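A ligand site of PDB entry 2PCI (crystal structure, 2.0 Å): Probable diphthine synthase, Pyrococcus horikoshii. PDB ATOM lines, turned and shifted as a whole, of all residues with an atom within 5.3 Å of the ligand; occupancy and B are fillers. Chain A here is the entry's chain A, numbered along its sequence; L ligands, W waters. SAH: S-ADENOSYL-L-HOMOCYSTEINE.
O of Pro 233 sits at hydrogen-bond distance from N of Arg 208, at 3.0 Å.
The side-chain hydroxyl (OG1) of Thr 92 sits at hydrogen-bond distance from the backbone carbonyl oxygen (O) of Pro 88.
O of Asp 167 sits at hydrogen-bond distance from N of Met 176, 3.2 Å away.
The side-chain hydroxyl (OG) of Ser 115 lies close to the backbone NH (N) of Tyr 117, 3.2 Å away.
The backbone NH of Ile 235 sits at hydrogen-bond distance from the backbone carbonyl oxygen of Leu 206 (3.0 Å).
O of Thr 36 sits close to SD of the ligand (3.5 Å).
Merely in contact with the ligand: Ser 37 (3.1 Å), Pro 85 (3.9 Å), Gly 86 (3.7 Å), Ala 91 (3.7 Å), Thr 92 (3.8 Å), Phe 165 (3.7 Å), Asp 167 (3.96 Å), Ile 168 (3.8 Å), Leu 206 (3.6 Å), Pro 233 (3.5 Å) and Ile 235 (3.0 Å).
Hydrophobic or aromatic side chains within 4 Å of the ligand: Leu 10, Val 90, Ala 91, Ile 116, Phe 165, Leu 166, Ile 168, Ala 209, Pro 233 and Ile 235.
Of the 29 residues printed, 21 come within 4 Å of the ligand.
The nearest printed residue that does not touch the ligand is Ala 207 (4.4 Å).
Water W2 lies within hydrogen-bond range of an oxygen (O3') of the ligand and the backbone carbonyl oxygen (O) of Asp 167.
Water W3 lies within hydrogen-bond range of a nitrogen (N) of the ligand (2.7 Å), the side-chain hydroxyl (OG1) of Thr 36 (2.8 Å) and the backbone carbonyl oxygen (O) of Pro 85 (2.9 Å).
OG of Ser 115 sits at hydrogen-bond distance from O of the ligand.
The backbone carbonyl oxygen (O) of Leu 10 is in hydrogen-bond range of a nitrogen (N6) of the ligand (3.2 Å).
OXT of the ligand sits at hydrogen-bond distance from N of Ile 116 (3.0 Å).
A nitrogen (N) of the ligand sits at hydrogen-bond distance from the backbone carbonyl oxygen of Val 90 (2.5 Å).
O of Leu 166 is in hydrogen-bond range of O3' of the ligand (2.6 Å).
A nitrogen (N6) of the ligand sits at hydrogen-bond distance from the backbone carbonyl oxygen (O) of Ala 209, at 2.8 Å.
A nitrogen (N1) of the ligand sits at hydrogen-bond distance from the backbone NH (N) of Ala 209.
The backbone NH (N) of Arg 208 lies within hydrogen-bond range of a nitrogen (N1) of the ligand (3.5 Å).
O of Asp 87 lies within hydrogen-bond range of N of the ligand, at 2.8 Å.
The backbone NH (N) of Leu 166 lies within hydrogen-bond range of an oxygen (O2') of the ligand, at 3.2 Å.
O of the ligand sits at hydrogen-bond distance from N of Asp 87, 2.8 Å away.
O of His 234 sits at hydrogen-bond distance from O2' of the ligand, 2.5 Å away.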
ATOM      1  N   LEU A  10     -23.059 -21.692   6.089  1.00  0.00           N
ATOM      2  CA  LEU A  10     -24.455 -21.250   6.209  1.00  0.00           C
ATOM      3  C   LEU A  10     -24.939 -21.030   7.651  1.00  0.00           C
ATOM      4  O   LEU A  10     -25.618 -20.068   7.964  1.00  0.00           O
ATOM      5  CB  LEU A  10     -25.345 -22.343   5.580  1.00  0.00           C
ATOM      6  CG  LEU A  10     -25.170 -22.477   4.066  1.00  0.00           C
ATOM      7  CD1 LEU A  10     -25.754 -23.789   3.536  1.00  0.00           C
ATOM      8  CD2 LEU A  10     -25.872 -21.360   3.295  1.00  0.00           C
ATOM      9  N   TYR A  11     -24.605 -22.003   8.535  1.00  0.00           N
ATOM     10  CA  TYR A  11     -25.302 -22.067   9.825  1.00  0.00           C
ATOM     11  C   TYR A  11     -24.373 -22.007  11.042  1.00  0.00           C
ATOM     12  O   TYR A  11     -24.500 -21.169  11.920  1.00  0.00           O
ATOM     13  CB  TYR A  11     -26.114 -23.367   9.847  1.00  0.00           C
ATOM     14  CG  TYR A  11     -26.948 -23.423  11.081  1.00  0.00           C
ATOM     15  CD1 TYR A  11     -27.888 -22.438  11.323  1.00  0.00           C
ATOM     16  CD2 TYR A  11     -26.803 -24.485  11.984  1.00  0.00           C
ATOM     17  CE1 TYR A  11     -28.693 -22.502  12.454  1.00  0.00           C
ATOM     18  CE2 TYR A  11     -27.599 -24.544  13.114  1.00  0.00           C
ATOM     19  CZ  TYR A  11     -28.531 -23.555  13.355  1.00  0.00           C
ATOM     20  OH  TYR A  11     -29.334 -23.602  14.487  1.00  0.00           O
ATOM     21  N   THR A  36     -22.763  -9.111   6.942  1.00  0.00           N
ATOM     22  CA  THR A  36     -23.336  -9.472   5.641  1.00  0.00           C
ATOM     23  C   THR A  36     -24.375 -10.578   5.746  1.00  0.00           C
ATOM     24  O   THR A  36     -25.186 -10.774   4.828  1.00  0.00           O
ATOM     25  CB  THR A  36     -22.251  -9.908   4.629  1.00  0.00           C
ATOM     26  OG1 THR A  36     -21.393 -10.879   5.243  1.00  0.00           O
ATOM     27  CG2 THR A  36     -21.436  -8.713   4.172  1.00  0.00           C
ATOM     28  N   SER A  37     -24.353 -11.302   6.851  1.00  0.00           N
ATOM     29  CA  SER A  37     -25.304 -12.383   7.047  1.00  0.00           C
ATOM     30  C   SER A  37     -25.311 -12.831   8.493  1.00  0.00           C
ATOM     31  O   SER A  37     -24.508 -12.373   9.301  1.00  0.00           O
ATOM     32  CB  SER A  37     -24.941 -13.566   6.146  1.00  0.00           C
ATOM     33  OG  SER A  37     -25.901 -14.606   6.251  1.00  0.00           O
ATOM     34  N   LEU A  38     -26.217 -13.743   8.820  1.00  0.00           N
ATOM     35  CA  LEU A  38     -26.338 -14.248  10.179  1.00  0.00           C
ATOM     36  C   LEU A  38     -26.091 -15.750  10.232  1.00  0.00           C
ATOM     37  O   LEU A  38     -26.726 -16.517   9.494  1.00  0.00           O
ATOM     38  CB  LEU A  38     -27.727 -13.947  10.738  1.00  0.00           C
ATOM     39  CG  LEU A  38     -28.116 -14.661  12.051  1.00  0.00           C
ATOM     40  CD1 LEU A  38     -27.206 -14.192  13.182  1.00  0.00           C
ATOM     41  CD2 LEU A  38     -29.572 -14.363  12.375  1.00  0.00           C
ATOM     42  N   PRO A  85     -19.484 -14.892   6.714  1.00  0.00           N
ATOM     43  CA  PRO A  85     -20.532 -15.916   6.722  1.00  0.00           C
ATOM     44  C   PRO A  85     -20.736 -16.386   5.280  1.00  0.00           C
ATOM     45  O   PRO A  85     -20.396 -15.662   4.342  1.00  0.00           O
ATOM     46  CB  PRO A  85     -21.759 -15.150   7.241  1.00  0.00           C
ATOM     47  CG  PRO A  85     -21.158 -14.043   8.051  1.00  0.00           C
ATOM     48  CD  PRO A  85     -19.992 -13.606   7.212  1.00  0.00           C
ATOM     49  N   GLY A  86     -21.290 -17.586   5.111  1.00  0.00           N
ATOM     50  CA  GLY A  86     -21.540 -18.121   3.772  1.00  0.00           C
ATOM     51  C   GLY A  86     -20.301 -18.069   2.886  1.00  0.00           C
ATOM     52  O   GLY A  86     -19.214 -18.432   3.326  1.00  0.00           O
ATOM     53  N   ASP A  87     -20.478 -17.648   1.637  1.00  0.00           N
ATOM     54  CA  ASP A  87     -19.371 -17.494   0.687  1.00  0.00           C
ATOM     55  C   ASP A  87     -19.035 -16.009   0.734  1.00  0.00           C
ATOM     56  O   ASP A  87     -19.930 -15.163   0.663  1.00  0.00           O
ATOM     57  CB  ASP A  87     -19.795 -17.894  -0.716  1.00  0.00           C
ATOM     58  CG  ASP A  87     -18.652 -17.774  -1.719  1.00  0.00           C
ATOM     59  OD1 ASP A  87     -18.229 -16.629  -2.007  1.00  0.00           O
ATOM     60  OD2 ASP A  87     -18.179 -18.812  -2.218  1.00  0.00           O
ATOM     61  N   PRO A  88     -17.738 -15.674   0.854  1.00  0.00           N
ATOM     62  CA  PRO A  88     -17.307 -14.275   0.911  1.00  0.00           C
ATOM     63  C   PRO A  88     -17.676 -13.328  -0.232  1.00  0.00           C
ATOM     64  O   PRO A  88     -17.807 -12.129  -0.011  1.00  0.00           O
ATOM     65  CB  PRO A  88     -15.799 -14.387   1.110  1.00  0.00           C
ATOM     66  CG  PRO A  88     -15.459 -15.690   0.445  1.00  0.00           C
ATOM     67  CD  PRO A  88     -16.590 -16.595   0.861  1.00  0.00           C
ATOM     68  N   VAL A  90     -20.437 -13.734  -2.379  1.00  0.00           N
ATOM     69  CA  VAL A  90     -21.829 -13.873  -2.800  1.00  0.00           C
ATOM     70  C   VAL A  90     -22.741 -12.909  -2.049  1.00  0.00           C
ATOM     71  O   VAL A  90     -22.893 -12.992  -0.832  1.00  0.00           O
ATOM     72  CB  VAL A  90     -22.335 -15.316  -2.593  1.00  0.00           C
ATOM     73  CG1 VAL A  90     -23.844 -15.361  -2.758  1.00  0.00           C
ATOM     74  CG2 VAL A  90     -21.662 -16.248  -3.602  1.00  0.00           C
ATOM     75  N   ALA A  91     -23.362 -11.993  -2.788  1.00  0.00           N
ATOM     76  CA  ALA A  91     -24.266 -11.012  -2.209  1.00  0.00           C
ATOM     77  C   ALA A  91     -23.562 -10.114  -1.193  1.00  0.00           C
ATOM     78  O   ALA A  91     -24.114  -9.800  -0.133  1.00  0.00           O
ATOM     79  CB  ALA A  91     -25.465 -11.713  -1.555  1.00  0.00           C
ATOM     80  N   THR A  92     -22.330  -9.743  -1.513  1.00  0.00           N
ATOM     81  CA  THR A  92     -21.522  -8.838  -0.692  1.00  0.00           C
ATOM     82  C   THR A  92     -20.769  -8.007  -1.730  1.00  0.00           C
ATOM     83  O   THR A  92     -20.911  -8.235  -2.920  1.00  0.00           O
ATOM     84  CB  THR A  92     -20.461  -9.576   0.151  1.00  0.00           C
ATOM     85  OG1 THR A  92     -19.438 -10.081  -0.719  1.00  0.00           O
ATOM     86  CG2 THR A  92     -21.070 -10.730   0.942  1.00  0.00           C
ATOM     87  N   PRO A 114     -20.255 -23.207   1.642  1.00  0.00           N
ATOM     88  CA  PRO A 114     -21.654 -23.252   1.209  1.00  0.00           C
ATOM     89  C   PRO A 114     -22.304 -21.869   1.297  1.00  0.00           C
ATOM     90  O   PRO A 114     -22.077 -21.116   2.249  1.00  0.00           O
ATOM     91  CB  PRO A 114     -22.287 -24.299   2.132  1.00  0.00           C
ATOM     92  CG  PRO A 114     -21.372 -24.365   3.312  1.00  0.00           C
ATOM     93  CD  PRO A 114     -19.989 -24.189   2.710  1.00  0.00           C
ATOM     94  N   SER A 115     -23.094 -21.543   0.283  1.00  0.00           N
ATOM     95  CA  SER A 115     -23.761 -20.245   0.180  1.00  0.00           C
ATOM     96  C   SER A 115     -25.267 -20.418   0.027  1.00  0.00           C
ATOM     97  O   SER A 115     -25.737 -21.412  -0.561  1.00  0.00           O
ATOM     98  CB  SER A 115     -23.210 -19.497  -1.037  1.00  0.00           C
ATOM     99  OG  SER A 115     -23.960 -18.329  -1.318  1.00  0.00           O
ATOM    100  N   ILE A 116     -26.034 -19.470   0.534  1.00  0.00           N
ATOM    101  CA  ILE A 116     -27.482 -19.574   0.426  1.00  0.00           C
ATOM    102  C   ILE A 116     -27.868 -19.583  -1.055  1.00  0.00           C
ATOM    103  O   ILE A 116     -28.868 -20.188  -1.438  1.00  0.00           O
ATOM    104  CB  ILE A 116     -28.198 -18.410   1.151  1.00  0.00           C
ATOM    105  CG1 ILE A 116     -29.706 -18.670   1.175  1.00  0.00           C
ATOM    106  CG2 ILE A 116     -27.873 -17.075   0.486  1.00  0.00           C
ATOM    107  CD1 ILE A 116     -30.102 -19.923   1.935  1.00  0.00           C
ATOM    108  N   TYR A 117     -27.053 -18.950  -1.896  1.00  0.00           N
ATOM    109  CA  TYR A 117     -27.337 -18.883  -3.322  1.00  0.00           C
ATOM    110  C   TYR A 117     -27.468 -20.250  -3.994  1.00  0.00           C
ATOM    111  O   TYR A 117     -28.251 -20.420  -4.936  1.00  0.00           O
ATOM    112  CB  TYR A 117     -26.260 -18.059  -4.039  1.00  0.00           C
ATOM    113  CG  TYR A 117     -26.650 -17.678  -5.451  1.00  0.00           C
ATOM    114  CD1 TYR A 117     -27.637 -16.717  -5.688  1.00  0.00           C
ATOM    115  CD2 TYR A 117     -26.066 -18.304  -6.553  1.00  0.00           C
ATOM    116  CE1 TYR A 117     -28.037 -16.399  -6.985  1.00  0.00           C
ATOM    117  CE2 TYR A 117     -26.447 -18.000  -7.845  1.00  0.00           C
ATOM    118  CZ  TYR A 117     -27.428 -17.045  -8.062  1.00  0.00           C
ATOM    119  OH  TYR A 117     -27.780 -16.750  -9.350  1.00  0.00           O
ATOM    120  N   PHE A 165     -33.034 -12.161  -1.321  1.00  0.00           N
ATOM    121  CA  PHE A 165     -32.217 -12.112  -0.121  1.00  0.00           C
ATOM    122  C   PHE A 165     -32.983 -11.135   0.778  1.00  0.00           C
ATOM    123  O   PHE A 165     -33.519 -10.141   0.286  1.00  0.00           O
ATOM    124  CB  PHE A 165     -30.842 -11.524  -0.447  1.00  0.00           C
ATOM    125  CG  PHE A 165     -29.961 -12.426  -1.286  1.00  0.00           C
ATOM    126  CD1 PHE A 165     -29.147 -13.381  -0.674  1.00  0.00           C
ATOM    127  CD2 PHE A 165     -29.952 -12.321  -2.665  1.00  0.00           C
ATOM    128  CE1 PHE A 165     -28.318 -14.202  -1.450  1.00  0.00           C
ATOM    129  CE2 PHE A 165     -29.135 -13.141  -3.447  1.00  0.00           C
ATOM    130  CZ  PHE A 165     -28.315 -14.085  -2.829  1.00  0.00           C
ATOM    131  N   LEU A 166     -33.068 -11.429   2.070  1.00  0.00           N
ATOM    132  CA  LEU A 166     -33.762 -10.536   2.996  1.00  0.00           C
ATOM    133  C   LEU A 166     -32.729  -9.662   3.721  1.00  0.00           C
ATOM    134  O   LEU A 166     -31.618 -10.114   4.015  1.00  0.00           O
ATOM    135  CB  LEU A 166     -34.604 -11.363   3.972  1.00  0.00           C
ATOM    136  CG  LEU A 166     -35.580 -12.295   3.262  1.00  0.00           C
ATOM    137  CD1 LEU A 166     -36.603 -12.841   4.240  1.00  0.00           C
ATOM    138  CD2 LEU A 166     -36.299 -11.542   2.140  1.00  0.00           C
ATOM    139  N   ASP A 167     -33.105  -8.425   3.997  1.00  0.00           N
ATOM    140  CA  ASP A 167     -32.205  -7.472   4.638  1.00  0.00           C
ATOM    141  C   ASP A 167     -31.729  -7.844   6.033  1.00  0.00           C
ATOM    142  O   ASP A 167     -32.335  -8.674   6.721  1.00  0.00           O
ATOM    143  CB  ASP A 167     -32.850  -6.084   4.682  1.00  0.00           C
ATOM    144  CG  ASP A 167     -31.834  -4.957   4.580  1.00  0.00           C
ATOM    145  OD1 ASP A 167     -30.612  -5.235   4.665  1.00  0.00           O
ATOM    146  OD2 ASP A 167     -32.241  -3.786   4.418  1.00  0.00           O
ATOM    147  N   ILE A 168     -30.637  -7.215   6.442  1.00  0.00           N
ATOM    148  CA  ILE A 168     -30.036  -7.438   7.747  1.00  0.00           C
ATOM    149  C   ILE A 168     -29.314  -6.175   8.219  1.00  0.00           C
ATOM    150  O   ILE A 168     -28.554  -5.572   7.462  1.00  0.00           O
ATOM    151  CB  ILE A 168     -29.023  -8.617   7.716  1.00  0.00           C
ATOM    152  CG1 ILE A 168     -28.195  -8.633   8.999  1.00  0.00           C
ATOM    153  CG2 ILE A 168     -28.104  -8.483   6.502  1.00  0.00           C
ATOM    154  CD1 ILE A 168     -27.202  -9.774   9.091  1.00  0.00           C
ATOM    155  N   MET A 176     -34.502  -9.468   8.886  1.00  0.00           N
ATOM    156  CA  MET A 176     -35.798  -9.553   8.228  1.00  0.00           C
ATOM    157  C   MET A 176     -36.317 -10.977   8.067  1.00  0.00           C
ATOM    158  O   MET A 176     -35.633 -11.847   7.520  1.00  0.00           O
ATOM    159  CB  MET A 176     -35.713  -8.881   6.855  1.00  0.00           C
ATOM    160  CG  MET A 176     -37.061  -8.757   6.155  1.00  0.00           C
ATOM    161  SD  MET A 176     -36.896  -8.007   4.532  1.00  0.00           S
ATOM    162  CE  MET A 176     -36.592  -6.292   4.969  1.00  0.00           C
ATOM    163  N   LEU A 206     -37.275 -20.538   3.020  1.00  0.00           N
ATOM    164  CA  LEU A 206     -36.205 -21.398   3.498  1.00  0.00           C
ATOM    165  C   LEU A 206     -35.557 -20.662   4.654  1.00  0.00           C
ATOM    166  O   LEU A 206     -35.023 -19.570   4.490  1.00  0.00           O
ATOM    167  CB  LEU A 206     -35.167 -21.643   2.395  1.00  0.00           C
ATOM    168  CG  LEU A 206     -33.886 -22.381   2.795  1.00  0.00           C
ATOM    169  CD1 LEU A 206     -34.247 -23.690   3.479  1.00  0.00           C
ATOM    170  CD2 LEU A 206     -33.020 -22.631   1.553  1.00  0.00           C
ATOM    171  N   ALA A 207     -35.618 -21.266   5.834  1.00  0.00           N
ATOM    172  CA  ALA A 207     -35.057 -20.655   7.033  1.00  0.00           C
ATOM    173  C   ALA A 207     -33.973 -21.517   7.638  1.00  0.00           C
ATOM    174  O   ALA A 207     -34.146 -22.718   7.819  1.00  0.00           O
ATOM    175  CB  ALA A 207     -36.155 -20.397   8.065  1.00  0.00           C
ATOM    176  N   ARG A 208     -32.851 -20.873   7.966  1.00  0.00           N
ATOM    177  CA  ARG A 208     -31.724 -21.542   8.590  1.00  0.00           C
ATOM    178  C   ARG A 208     -31.163 -22.694   7.761  1.00  0.00           C
ATOM    179  O   ARG A 208     -30.969 -23.796   8.259  1.00  0.00           O
ATOM    180  CB  ARG A 208     -32.125 -22.034   9.985  1.00  0.00           C
ATOM    181  CG  ARG A 208     -32.652 -20.926  10.903  1.00  0.00           C
ATOM    182  CD  ARG A 208     -33.052 -21.488  12.262  1.00  0.00           C
ATOM    183  NE  ARG A 208     -33.968 -22.608  12.140  1.00  0.00           N
ATOM    184  CZ  ARG A 208     -35.230 -22.505  11.715  1.00  0.00           C
ATOM    185  NH1 ARG A 208     -35.725 -21.330  11.385  1.00  0.00           N
ATOM    186  NH2 ARG A 208     -35.979 -23.591  11.612  1.00  0.00           N
ATOM    187  N   ALA A 209     -30.902 -22.425   6.484  1.00  0.00           N
ATOM    188  CA  ALA A 209     -30.322 -23.451   5.626  1.00  0.00           C
ATOM    189  C   ALA A 209     -28.969 -23.762   6.266  1.00  0.00           C
ATOM    190  O   ALA A 209     -28.351 -22.889   6.858  1.00  0.00           O
ATOM    191  CB  ALA A 209     -30.142 -22.918   4.212  1.00  0.00           C
ATOM    192  N   GLY A 210     -28.504 -25.003   6.157  1.00  0.00           N
ATOM    193  CA  GLY A 210     -27.227 -25.328   6.755  1.00  0.00           C
ATOM    194  C   GLY A 210     -27.437 -26.119   8.034  1.00  0.00           C
ATOM    195  O   GLY A 210     -26.618 -26.964   8.397  1.00  0.00           O
ATOM    196  N   PRO A 233     -31.602 -16.701   9.961  1.00  0.00           N
ATOM    197  CA  PRO A 233     -32.005 -15.994   8.747  1.00  0.00           C
ATOM    198  C   PRO A 233     -33.051 -16.722   7.912  1.00  0.00           C
ATOM    199  O   PRO A 233     -33.199 -17.943   7.998  1.00  0.00           O
ATOM    200  CB  PRO A 233     -30.688 -15.829   8.010  1.00  0.00           C
ATOM    201  CG  PRO A 233     -29.985 -17.108   8.338  1.00  0.00           C
ATOM    202  CD  PRO A 233     -30.254 -17.266   9.816  1.00  0.00           C
ATOM    203  N   HIS A 234     -33.751 -15.948   7.087  1.00  0.00           N
ATOM    204  CA  HIS A 234     -34.773 -16.463   6.181  1.00  0.00           C
ATOM    205  C   HIS A 234     -34.508 -15.933   4.786  1.00  0.00           C
ATOM    206  O   HIS A 234     -33.926 -14.864   4.630  1.00  0.00           O
ATOM    207  CB  HIS A 234     -36.171 -15.951   6.565  1.00  0.00           C
ATOM    208  CG  HIS A 234     -36.665 -16.433   7.893  1.00  0.00           C
ATOM    209  ND1 HIS A 234     -37.907 -16.078   8.380  1.00  0.00           N
ATOM    210  CD2 HIS A 234     -36.106 -17.244   8.818  1.00  0.00           C
ATOM    211  CE1 HIS A 234     -38.088 -16.651   9.559  1.00  0.00           C
ATOM    212  NE2 HIS A 234     -37.019 -17.360   9.847  1.00  0.00           N
ATOM    213  N   ILE A 235     -34.927 -16.682   3.776  1.00  0.00           N
ATOM    214  CA  ILE A 235     -34.826 -16.227   2.398  1.00  0.00           C
ATOM    215  C   ILE A 235     -36.198 -16.490   1.817  1.00  0.00           C
ATOM    216  O   ILE A 235     -36.883 -17.432   2.235  1.00  0.00           O
ATOM    217  CB  ILE A 235     -33.800 -16.982   1.531  1.00  0.00           C
ATOM    218  CG1 ILE A 235     -34.108 -18.471   1.524  1.00  0.00           C
ATOM    219  CG2 ILE A 235     -32.406 -16.676   2.004  1.00  0.00           C
ATOM    220  CD1 ILE A 235     -33.608 -19.174   0.295  1.00  0.00           C
HETATM  221  N   SAH L   1     -22.459 -14.290   1.303  1.00  0.00           N
HETATM  222  CA  SAH L   1     -23.609 -14.979   2.044  1.00  0.00           C
HETATM  223  CB  SAH L   1     -24.938 -14.265   2.061  1.00  0.00           C
HETATM  224  CG  SAH L   1     -24.974 -12.757   1.970  1.00  0.00           C
HETATM  225  SD  SAH L   1     -26.730 -12.212   2.067  1.00  0.00           S
HETATM  226  C   SAH L   1     -23.752 -16.420   1.415  1.00  0.00           C
HETATM  227  O   SAH L   1     -22.947 -16.786   0.527  1.00  0.00           O
HETATM  228  OXT SAH L   1     -24.715 -17.164   1.879  1.00  0.00           O
HETATM  229  C5' SAH L   1     -27.323 -12.608   3.691  1.00  0.00           C
HETATM  230  C4' SAH L   1     -28.911 -12.777   3.654  1.00  0.00           C
HETATM  231  O4' SAH L   1     -29.247 -14.012   2.934  1.00  0.00           O
HETATM  232  C3' SAH L   1     -29.550 -12.872   5.002  1.00  0.00           C
HETATM  233  O3' SAH L   1     -29.979 -11.594   5.441  1.00  0.00           O
HETATM  234  C2' SAH L   1     -30.702 -13.914   4.800  1.00  0.00           C
HETATM  235  O2' SAH L   1     -31.921 -13.310   4.384  1.00  0.00           O
HETATM  236  C1' SAH L   1     -30.114 -14.947   3.763  1.00  0.00           C
HETATM  237  N9  SAH L   1     -29.360 -16.057   4.279  1.00  0.00           N
HETATM  238  C8  SAH L   1     -28.040 -16.154   4.626  1.00  0.00           C
HETATM  239  N7  SAH L   1     -27.659 -17.358   4.926  1.00  0.00           N
HETATM  240  C5  SAH L   1     -28.896 -18.054   5.107  1.00  0.00           C
HETATM  241  C6  SAH L   1     -29.193 -19.335   5.671  1.00  0.00           C
HETATM  242  N6  SAH L   1     -28.270 -20.150   6.194  1.00  0.00           N
HETATM  243  N1  SAH L   1     -30.532 -19.677   5.661  1.00  0.00           N
HETATM  244  C2  SAH L   1     -31.511 -18.884   5.137  1.00  0.00           C
HETATM  245  N3  SAH L   1     -31.259 -17.639   4.613  1.00  0.00           N
HETATM  246  C4  SAH L   1     -29.934 -17.284   4.674  1.00  0.00           C
HETATM  247  O   HOH W   1     -24.941 -17.880   4.576  1.00  0.00           O
HETATM  248  O   HOH W   2     -31.446 -11.414   7.636  1.00  0.00           O
HETATM  249  O   HOH W   3     -21.682 -13.169   3.595  1.00  0.00           O
